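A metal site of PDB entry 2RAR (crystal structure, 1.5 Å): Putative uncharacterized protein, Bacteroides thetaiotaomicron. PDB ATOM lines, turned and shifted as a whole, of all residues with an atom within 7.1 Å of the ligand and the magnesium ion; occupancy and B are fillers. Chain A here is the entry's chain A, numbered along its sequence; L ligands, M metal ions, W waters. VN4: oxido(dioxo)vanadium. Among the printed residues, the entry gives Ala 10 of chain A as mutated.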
ATOM      1  N   PHE A   7      19.725 -19.616  18.281  1.00  0.00           N
ATOM      2  CA  PHE A   7      18.843 -20.738  18.573  1.00  0.00           C
ATOM      3  C   PHE A   7      19.271 -21.580  19.773  1.00  0.00           C
ATOM      4  O   PHE A   7      20.395 -22.146  19.787  1.00  0.00           O
ATOM      5  CB  PHE A   7      18.864 -21.725  17.383  1.00  0.00           C
ATOM      6  CG  PHE A   7      18.260 -21.173  16.099  1.00  0.00           C
ATOM      7  CD1 PHE A   7      19.082 -20.621  15.092  1.00  0.00           C
ATOM      8  CD2 PHE A   7      16.863 -21.178  15.930  1.00  0.00           C
ATOM      9  CE1 PHE A   7      18.553 -20.092  13.930  1.00  0.00           C
ATOM     10  CE2 PHE A   7      16.260 -20.639  14.803  1.00  0.00           C
ATOM     11  CZ  PHE A   7      17.093 -20.082  13.760  1.00  0.00           C
ATOM     12  N   ASP A   8      18.343 -21.751  20.708  1.00  0.00           N
ATOM     13  CA  ASP A   8      18.534 -22.776  21.721  1.00  0.00           C
ATOM     14  C   ASP A   8      18.478 -24.150  21.011  1.00  0.00           C
ATOM     15  O   ASP A   8      17.903 -24.292  19.933  1.00  0.00           O
ATOM     16  CB  ASP A   8      17.360 -22.660  22.753  1.00  0.00           C
ATOM     17  CG  ASP A   8      17.337 -23.792  23.751  1.00  0.00           C
ATOM     18  OD1 ASP A   8      16.292 -24.447  23.897  1.00  0.00           O
ATOM     19  OD2 ASP A   8      18.445 -23.953  24.304  1.00  0.00           O
ATOM     20  N   ILE A   9      19.038 -25.188  21.653  1.00  0.00           N
ATOM     21  CA  ILE A   9      19.012 -26.525  21.033  1.00  0.00           C
ATOM     22  C   ILE A   9      17.820 -27.297  21.586  1.00  0.00           C
ATOM     23  O   ILE A   9      16.835 -27.514  20.832  1.00  0.00           O
ATOM     24  CB  ILE A   9      20.280 -27.324  21.304  1.00  0.00           C
ATOM     25  CG1 ILE A   9      21.483 -26.578  20.794  1.00  0.00           C
ATOM     26  CG2 ILE A   9      20.101 -28.700  20.637  1.00  0.00           C
ATOM     27  CD1 ILE A   9      22.873 -27.389  21.212  1.00  0.00           C
ATOM     28  N   ALA A  10      17.831 -27.800  22.821  1.00  0.00           N
ATOM     29  CA  ALA A  10      16.754 -28.675  23.255  1.00  0.00           C
ATOM     30  C   ALA A  10      15.361 -28.050  23.336  1.00  0.00           C
ATOM     31  O   ALA A  10      15.226 -27.093  23.995  1.00  0.00           O
ATOM     32  CB  ALA A  10      17.195 -29.235  24.718  1.00  0.00           C
ATOM     33  N   GLY A  11      14.407 -28.570  22.585  1.00  0.00           N
ATOM     34  CA  GLY A  11      13.016 -28.089  22.563  1.00  0.00           C
ATOM     35  C   GLY A  11      12.861 -26.921  21.629  1.00  0.00           C
ATOM     36  O   GLY A  11      11.787 -26.406  21.503  1.00  0.00           O
ATOM     37  N   THR A  12      13.986 -26.498  20.966  1.00  0.00           N
ATOM     38  CA  THR A  12      13.854 -25.347  20.048  1.00  0.00           C
ATOM     39  C   THR A  12      14.321 -25.802  18.659  1.00  0.00           C
ATOM     40  O   THR A  12      13.544 -25.753  17.681  1.00  0.00           O
ATOM     41  CB  THR A  12      14.687 -24.201  20.606  1.00  0.00           C
ATOM     42  OG1 THR A  12      14.183 -23.789  21.865  1.00  0.00           O
ATOM     43  CG2 THR A  12      14.731 -23.025  19.632  1.00  0.00           C
ATOM     44  N   LEU A  13      15.577 -26.308  18.550  1.00  0.00           N
ATOM     45  CA  LEU A  13      15.998 -26.983  17.309  1.00  0.00           C
ATOM     46  C   LEU A  13      15.656 -28.470  17.383  1.00  0.00           C
ATOM     47  O   LEU A  13      15.252 -29.048  16.363  1.00  0.00           O
ATOM     48  CB  LEU A  13      17.544 -26.900  17.055  1.00  0.00           C
ATOM     49  CG  LEU A  13      17.871 -25.455  16.761  1.00  0.00           C
ATOM     50  CD1 LEU A  13      19.493 -25.367  16.769  1.00  0.00           C
ATOM     51  CD2 LEU A  13      17.325 -24.972  15.370  1.00  0.00           C
ATOM     52  N   VAL A  14      15.942 -29.126  18.518  1.00  0.00           N
ATOM     53  CA  VAL A  14      15.822 -30.629  18.647  1.00  0.00           C
ATOM     54  C   VAL A  14      14.659 -30.975  19.509  1.00  0.00           C
ATOM     55  O   VAL A  14      14.472 -30.540  20.603  1.00  0.00           O
ATOM     56  CB  VAL A  14      17.154 -31.176  19.286  1.00  0.00           C
ATOM     57  CG1 VAL A  14      17.056 -32.767  19.307  1.00  0.00           C
ATOM     58  CG2 VAL A  14      18.291 -30.880  18.326  1.00  0.00           C
ATOM     59  N   PHE A  16      12.265 -32.908  22.000  1.00  0.00           N
ATOM     60  CA  PHE A  16      12.470 -33.819  23.171  1.00  0.00           C
ATOM     61  C   PHE A  16      11.736 -35.129  22.899  1.00  0.00           C
ATOM     62  O   PHE A  16      12.107 -36.170  23.449  1.00  0.00           O
ATOM     63  CB  PHE A  16      11.892 -33.192  24.379  1.00  0.00           C
ATOM     64  CG  PHE A  16      12.786 -32.181  25.031  1.00  0.00           C
ATOM     65  CD1 PHE A  16      13.911 -32.600  25.732  1.00  0.00           C
ATOM     66  CD2 PHE A  16      12.440 -30.807  25.090  1.00  0.00           C
ATOM     67  CE1 PHE A  16      14.675 -31.666  26.491  1.00  0.00           C
ATOM     68  CE2 PHE A  16      13.164 -29.890  25.795  1.00  0.00           C
ATOM     69  CZ  PHE A  16      14.321 -30.340  26.527  1.00  0.00           C
ATOM     70  N   ILE A  41      24.239 -20.992  17.653  1.00  0.00           N
ATOM     71  CA  ILE A  41      23.661 -21.859  18.684  1.00  0.00           C
ATOM     72  C   ILE A  41      23.825 -21.139  20.012  1.00  0.00           C
ATOM     73  O   ILE A  41      24.835 -20.513  20.292  1.00  0.00           O
ATOM     74  CB  ILE A  41      24.473 -23.154  18.652  1.00  0.00           C
ATOM     75  CG1 ILE A  41      24.305 -23.861  17.330  1.00  0.00           C
ATOM     76  CG2 ILE A  41      24.098 -23.986  19.967  1.00  0.00           C
ATOM     77  CD1 ILE A  41      22.825 -24.285  17.047  1.00  0.00           C
ATOM     78  N   ALA A  42      22.832 -21.224  20.884  1.00  0.00           N
ATOM     79  CA  ALA A  42      22.906 -20.589  22.243  1.00  0.00           C
ATOM     80  C   ALA A  42      22.302 -21.632  23.186  1.00  0.00           C
ATOM     81  O   ALA A  42      21.079 -21.799  23.330  1.00  0.00           O
ATOM     82  CB  ALA A  42      22.142 -19.231  22.310  1.00  0.00           C
ATOM     83  N   THR A  43      23.235 -22.332  23.887  1.00  0.00           N
ATOM     84  CA  THR A  43      22.749 -23.518  24.694  1.00  0.00           C
ATOM     85  C   THR A  43      23.396 -23.533  26.048  1.00  0.00           C
ATOM     86  O   THR A  43      24.536 -23.043  26.255  1.00  0.00           O
ATOM     87  CB  THR A  43      23.162 -24.757  23.902  1.00  0.00           C
ATOM     88  OG1 THR A  43      22.751 -25.962  24.581  1.00  0.00           O
ATOM     89  CG2 THR A  43      24.689 -24.921  23.686  1.00  0.00           C
ATOM     90  N   GLY A  44      22.696 -24.229  26.941  1.00  0.00           N
ATOM     91  CA  GLY A  44      23.236 -24.498  28.277  1.00  0.00           C
ATOM     92  C   GLY A  44      24.244 -25.670  28.169  1.00  0.00           C
ATOM     93  O   GLY A  44      25.078 -25.784  29.082  1.00  0.00           O
ATOM     94  N   ARG A  45      24.294 -26.457  27.123  1.00  0.00           N
ATOM     95  CA  ARG A  45      25.266 -27.531  27.042  1.00  0.00           C
ATOM     96  C   ARG A  45      26.686 -27.076  26.754  1.00  0.00           C
ATOM     97  O   ARG A  45      26.908 -26.054  26.078  1.00  0.00           O
ATOM     98  CB  ARG A  45      24.964 -28.445  25.805  1.00  0.00           C
ATOM     99  CG  ARG A  45      23.617 -29.172  25.961  1.00  0.00           C
ATOM    100  CD  ARG A  45      23.592 -30.062  24.713  1.00  0.00           C
ATOM    101  NE  ARG A  45      22.274 -30.698  24.656  1.00  0.00           N
ATOM    102  CZ  ARG A  45      22.025 -31.983  24.434  1.00  0.00           C
ATOM    103  NH1 ARG A  45      23.044 -32.813  24.206  1.00  0.00           N
ATOM    104  NH2 ARG A  45      20.735 -32.392  24.563  1.00  0.00           N
ATOM    105  N   ASN A  52      23.975 -33.668  19.031  1.00  0.00           N
ATOM    106  CA  ASN A  52      22.716 -33.762  18.292  1.00  0.00           C
ATOM    107  C   ASN A  52      22.471 -32.733  17.206  1.00  0.00           C
ATOM    108  O   ASN A  52      21.385 -32.558  16.721  1.00  0.00           O
ATOM    109  CB  ASN A  52      21.565 -33.715  19.296  1.00  0.00           C
ATOM    110  CG  ASN A  52      21.614 -32.482  20.216  1.00  0.00           C
ATOM    111  OD1 ASN A  52      22.552 -31.684  20.161  1.00  0.00           O
ATOM    112  ND2 ASN A  52      20.607 -32.359  21.124  1.00  0.00           N
ATOM    113  N   ASN A  69      25.657 -21.608  28.633  1.00  0.00           N
ATOM    114  CA  ASN A  69      24.846 -20.426  29.003  1.00  0.00           C
ATOM    115  C   ASN A  69      25.604 -19.117  28.850  1.00  0.00           C
ATOM    116  O   ASN A  69      25.263 -18.188  29.569  1.00  0.00           O
ATOM    117  CB  ASN A  69      24.237 -20.584  30.417  1.00  0.00           C
ATOM    118  CG  ASN A  69      23.335 -21.787  30.452  1.00  0.00           C
ATOM    119  OD1 ASN A  69      22.269 -21.763  29.789  1.00  0.00           O
ATOM    120  ND2 ASN A  69      23.825 -22.904  31.077  1.00  0.00           N
ATOM    121  N   ARG A 173      17.624 -23.115  34.311  1.00  0.00           N
ATOM    122  CA  ARG A 173      17.294 -24.481  33.857  1.00  0.00           C
ATOM    123  C   ARG A 173      16.739 -24.577  32.456  1.00  0.00           C
ATOM    124  O   ARG A 173      16.045 -23.628  32.056  1.00  0.00           O
ATOM    125  CB  ARG A 173      16.165 -25.097  34.742  1.00  0.00           C
ATOM    126  CG  ARG A 173      16.446 -25.069  36.226  1.00  0.00           C
ATOM    127  CD  ARG A 173      15.391 -25.954  36.987  1.00  0.00           C
ATOM    128  NE  ARG A 173      15.707 -25.806  38.419  1.00  0.00           N
ATOM    129  CZ  ARG A 173      16.170 -26.799  39.191  1.00  0.00           C
ATOM    130  NH1 ARG A 173      16.340 -28.023  38.791  1.00  0.00           N
ATOM    131  NH2 ARG A 173      16.621 -26.445  40.408  1.00  0.00           N
ATOM    132  N   TRP A 174      17.166 -25.593  31.701  1.00  0.00           N
ATOM    133  CA  TRP A 174      16.566 -25.878  30.370  1.00  0.00           C
ATOM    134  C   TRP A 174      15.804 -27.206  30.477  1.00  0.00           C
ATOM    135  O   TRP A 174      15.174 -27.648  29.506  1.00  0.00           O
ATOM    136  CB  TRP A 174      17.570 -25.985  29.218  1.00  0.00           C
ATOM    137  CG  TRP A 174      18.888 -26.832  29.515  1.00  0.00           C
ATOM    138  CD1 TRP A 174      20.087 -26.381  30.146  1.00  0.00           C
ATOM    139  CD2 TRP A 174      19.165 -28.130  29.051  1.00  0.00           C
ATOM    140  NE1 TRP A 174      21.059 -27.344  30.074  1.00  0.00           N
ATOM    141  CE2 TRP A 174      20.550 -28.440  29.383  1.00  0.00           C
ATOM    142  CE3 TRP A 174      18.404 -29.045  28.338  1.00  0.00           C
ATOM    143  CZ2 TRP A 174      21.150 -29.649  29.019  1.00  0.00           C
ATOM    144  CZ3 TRP A 174      19.014 -30.274  27.938  1.00  0.00           C
ATOM    145  CH2 TRP A 174      20.394 -30.552  28.301  1.00  0.00           C
ATOM    146  N   TYR A 175      15.803 -27.838  31.669  1.00  0.00           N
ATOM    147  CA  TYR A 175      15.038 -29.095  31.845  1.00  0.00           C
ATOM    148  C   TYR A 175      14.773 -29.021  33.331  1.00  0.00           C
ATOM    149  O   TYR A 175      15.630 -28.629  34.099  1.00  0.00           O
ATOM    150  CB  TYR A 175      15.879 -30.292  31.392  1.00  0.00           C
ATOM    151  CG  TYR A 175      15.018 -31.533  31.395  1.00  0.00           C
ATOM    152  CD1 TYR A 175      14.179 -31.797  30.302  1.00  0.00           C
ATOM    153  CD2 TYR A 175      15.018 -32.420  32.507  1.00  0.00           C
ATOM    154  CE1 TYR A 175      13.343 -32.923  30.288  1.00  0.00           C
ATOM    155  CE2 TYR A 175      14.184 -33.535  32.521  1.00  0.00           C
ATOM    156  CZ  TYR A 175      13.343 -33.789  31.392  1.00  0.00           C
ATOM    157  OH  TYR A 175      12.532 -34.915  31.344  1.00  0.00           O
ATOM    158  N   ASP A 180      21.922 -25.401  35.657  1.00  0.00           N
ATOM    159  CA  ASP A 180      23.306 -25.044  35.281  1.00  0.00           C
ATOM    160  C   ASP A 180      23.692 -23.799  36.008  1.00  0.00           C
ATOM    161  O   ASP A 180      22.965 -22.811  36.115  1.00  0.00           O
ATOM    162  CB  ASP A 180      23.460 -24.726  33.762  1.00  0.00           C
ATOM    163  CG  ASP A 180      23.197 -25.876  32.890  1.00  0.00           C
ATOM    164  OD1 ASP A 180      23.545 -27.031  33.163  1.00  0.00           O
ATOM    165  OD2 ASP A 180      22.590 -25.568  31.792  1.00  0.00           O
ATOM    166  N   LYS A 188      22.784 -16.399  28.489  1.00  0.00           N
ATOM    167  CA  LYS A 188      22.813 -16.311  27.009  1.00  0.00           C
ATOM    168  C   LYS A 188      22.736 -14.897  26.532  1.00  0.00           C
ATOM    169  O   LYS A 188      23.142 -14.630  25.382  1.00  0.00           O
ATOM    170  CB  LYS A 188      21.651 -17.132  26.419  1.00  0.00           C
ATOM    171  CG  LYS A 188      21.809 -18.670  26.702  1.00  0.00           C
ATOM    172  CD  LYS A 188      20.636 -19.475  26.139  1.00  0.00           C
ATOM    173  CE  LYS A 188      20.766 -20.924  26.637  1.00  0.00           C
ATOM    174  NZ  LYS A 188      19.770 -21.783  25.931  1.00  0.00           N
ATOM    175  N   GLY A 210      13.695 -19.746  21.750  1.00  0.00           N
ATOM    176  CA  GLY A 210      13.940 -20.561  22.932  1.00  0.00           C
ATOM    177  C   GLY A 210      12.646 -21.202  23.439  1.00  0.00           C
ATOM    178  O   GLY A 210      11.543 -20.845  23.022  1.00  0.00           O
ATOM    179  N   ASP A 211      12.829 -22.186  24.316  1.00  0.00           N
ATOM    180  CA  ASP A 211      11.662 -22.859  24.912  1.00  0.00           C
ATOM    181  C   ASP A 211      11.764 -22.945  26.468  1.00  0.00           C
ATOM    182  O   ASP A 211      10.766 -23.471  27.056  1.00  0.00           O
ATOM    183  CB  ASP A 211      11.590 -24.312  24.398  1.00  0.00           C
ATOM    184  CG  ASP A 211      12.632 -25.171  24.994  1.00  0.00           C
ATOM    185  OD1 ASP A 211      13.804 -24.747  25.041  1.00  0.00           O
ATOM    186  OD2 ASP A 211      12.341 -26.255  25.603  1.00  0.00           O
ATOM    187  N   GLY A 212      12.855 -22.559  27.047  1.00  0.00           N
ATOM    188  CA  GLY A 212      13.171 -22.852  28.475  1.00  0.00           C
ATOM    189  C   GLY A 212      13.529 -21.643  29.338  1.00  0.00           C
ATOM    190  O   GLY A 212      13.723 -20.549  28.895  1.00  0.00           O
ATOM    191  N   GLY A 213      13.504 -21.857  30.664  1.00  0.00           N
ATOM    192  CA  GLY A 213      13.857 -20.788  31.573  1.00  0.00           C
ATOM    193  C   GLY A 213      15.234 -20.165  31.316  1.00  0.00           C
ATOM    194  O   GLY A 213      15.379 -18.957  31.481  1.00  0.00           O
ATOM    195  N   ASN A 214      16.192 -20.987  30.906  1.00  0.00           N
ATOM    196  CA  ASN A 214      17.494 -20.394  30.613  1.00  0.00           C
ATOM    197  C   ASN A 214      17.561 -19.612  29.279  1.00  0.00           C
ATOM    198  O   ASN A 214      18.627 -19.059  28.957  1.00  0.00           O
ATOM    199  CB  ASN A 214      18.657 -21.464  30.625  1.00  0.00           C
ATOM    200  CG  ASN A 214      18.591 -22.436  29.468  1.00  0.00           C
ATOM    201  OD1 ASN A 214      17.497 -22.614  28.880  1.00  0.00           O
ATOM    202  ND2 ASN A 214      19.616 -23.029  29.099  1.00  0.00           N
ATOM    203  N   ASP A 215      16.391 -19.471  28.631  1.00  0.00           N
ATOM    204  CA  ASP A 215      16.340 -18.668  27.395  1.00  0.00           C
ATOM    205  C   ASP A 215      15.650 -17.381  27.713  1.00  0.00           C
ATOM    206  O   ASP A 215      15.624 -16.477  26.877  1.00  0.00           O
ATOM    207  CB  ASP A 215      15.450 -19.389  26.331  1.00  0.00           C
ATOM    208  CG  ASP A 215      16.045 -20.694  25.876  1.00  0.00           C
ATOM    209  OD1 ASP A 215      17.281 -20.680  25.654  1.00  0.00           O
ATOM    210  OD2 ASP A 215      15.331 -21.677  25.751  1.00  0.00           O
HETATM  211  V   VN4 L   1      19.099 -25.411  25.512  1.00  0.00           V
HETATM  212  O1  VN4 L   1      19.918 -24.528  26.699  1.00  0.00           O
HETATM  213  O2  VN4 L   1      20.033 -26.214  24.348  1.00  0.00           O
HETATM  214  O3  VN4 L   1      17.583 -26.229  25.859  1.00  0.00           O
HETATM  215 MG    MG M   1      15.654 -25.586  25.499  1.00  0.00          MG
HETATM  216  O   HOH W   1      20.441 -28.845  25.536  1.00  0.00           O
HETATM  217  O   HOH W   2      16.004 -23.923  26.794  1.00  0.00           O
HETATM  218  O   HOH W   3      14.727 -26.828  26.852  1.00  0.00           O
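The magnesium ion is bound by water W3 (2.1 Å).
The magnesium ion is bound by O3 of the ligand (2.1 Å).
The magnesium ion is bound by OD1 of Asp 8 (2.1 Å).
The magnesium ion is bound by OD1 of Asp 211.
Water W2 binds the magnesium ion.
The magnesium ion is bound by O of Ala 10 (2.2 Å).
N of Ile 9 lies close to O2 of the ligand (3.1 Å).
O1 of the ligand sits close to N of Gly 44, 2.8 Å away.
An oxygen (O1) of the ligand sits close to the side-chain amino group (NZ) of Lys 188 (2.9 Å).
O1 of the ligand sits close to ND2 of Asn 214 (2.8 Å).
Merely in contact with the ligand: Trp 174 (3.4 Å).
Hydrophobic or aromatic side chains that line the ligand: Ile 9, Ala 10 and Trp 174.
Eight residues have an atom within 4 Å of the ligand: Asp 8, Ile 9, Ala 10, Thr 43, Gly 44, Trp 174, Lys 188 and Asn 214.
The side-chain carboxylate (OD2) of Asp 8 lies close to the side-chain amino group (NZ) of Lys 188.
OD1 of Asp 8 lies close to OG1 of Thr 12 (3.0 Å).
The backbone NH (N) of Leu 13 is in hydrogen-bond range of the backbone carbonyl oxygen (O) of Asp 8, at 3.4 Å.
N of Asp 211 sits at hydrogen-bond distance from OD2 of Asp 215 (2.9 Å).
The side-chain amide nitrogen of Asn 214 sits close to the side-chain amino group of Lys 188 (3.4 Å).
OD1 of Asn 69 is in hydrogen-bond range of ND2 of Asn 214 (3.0 Å).
N of Asn 214 lies within hydrogen-bond range of O of Arg 173 (2.9 Å).
OD2 of Asp 215 sits at hydrogen-bond distance from N of Gly 212, 2.9 Å away.
Water W2 lies within hydrogen-bond range of the side-chain carboxylate of Asp 215 (2.6 Å), the side-chain amide oxygen of Asn 214 (2.9 Å) and the backbone NH of Gly 212 (3.4 Å).
Water W3 bridges the side-chain carboxylate of Asp 211 (2.8 Å) and the backbone carbonyl oxygen of Trp 174 (2.8 Å).
Merely in contact with the magnesium ion: Asp 215.
Of the 27 residues printed, 4 come within 4 Å of the magnesium ion.
A vanadium atom (V) of the ligand is bound by the side-chain carboxylate (OD2) of Asp 8 (2.0 Å).
An oxygen (O2) of the ligand lies close to the side-chain hydroxyl of Thr 43 (2.7 Å).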
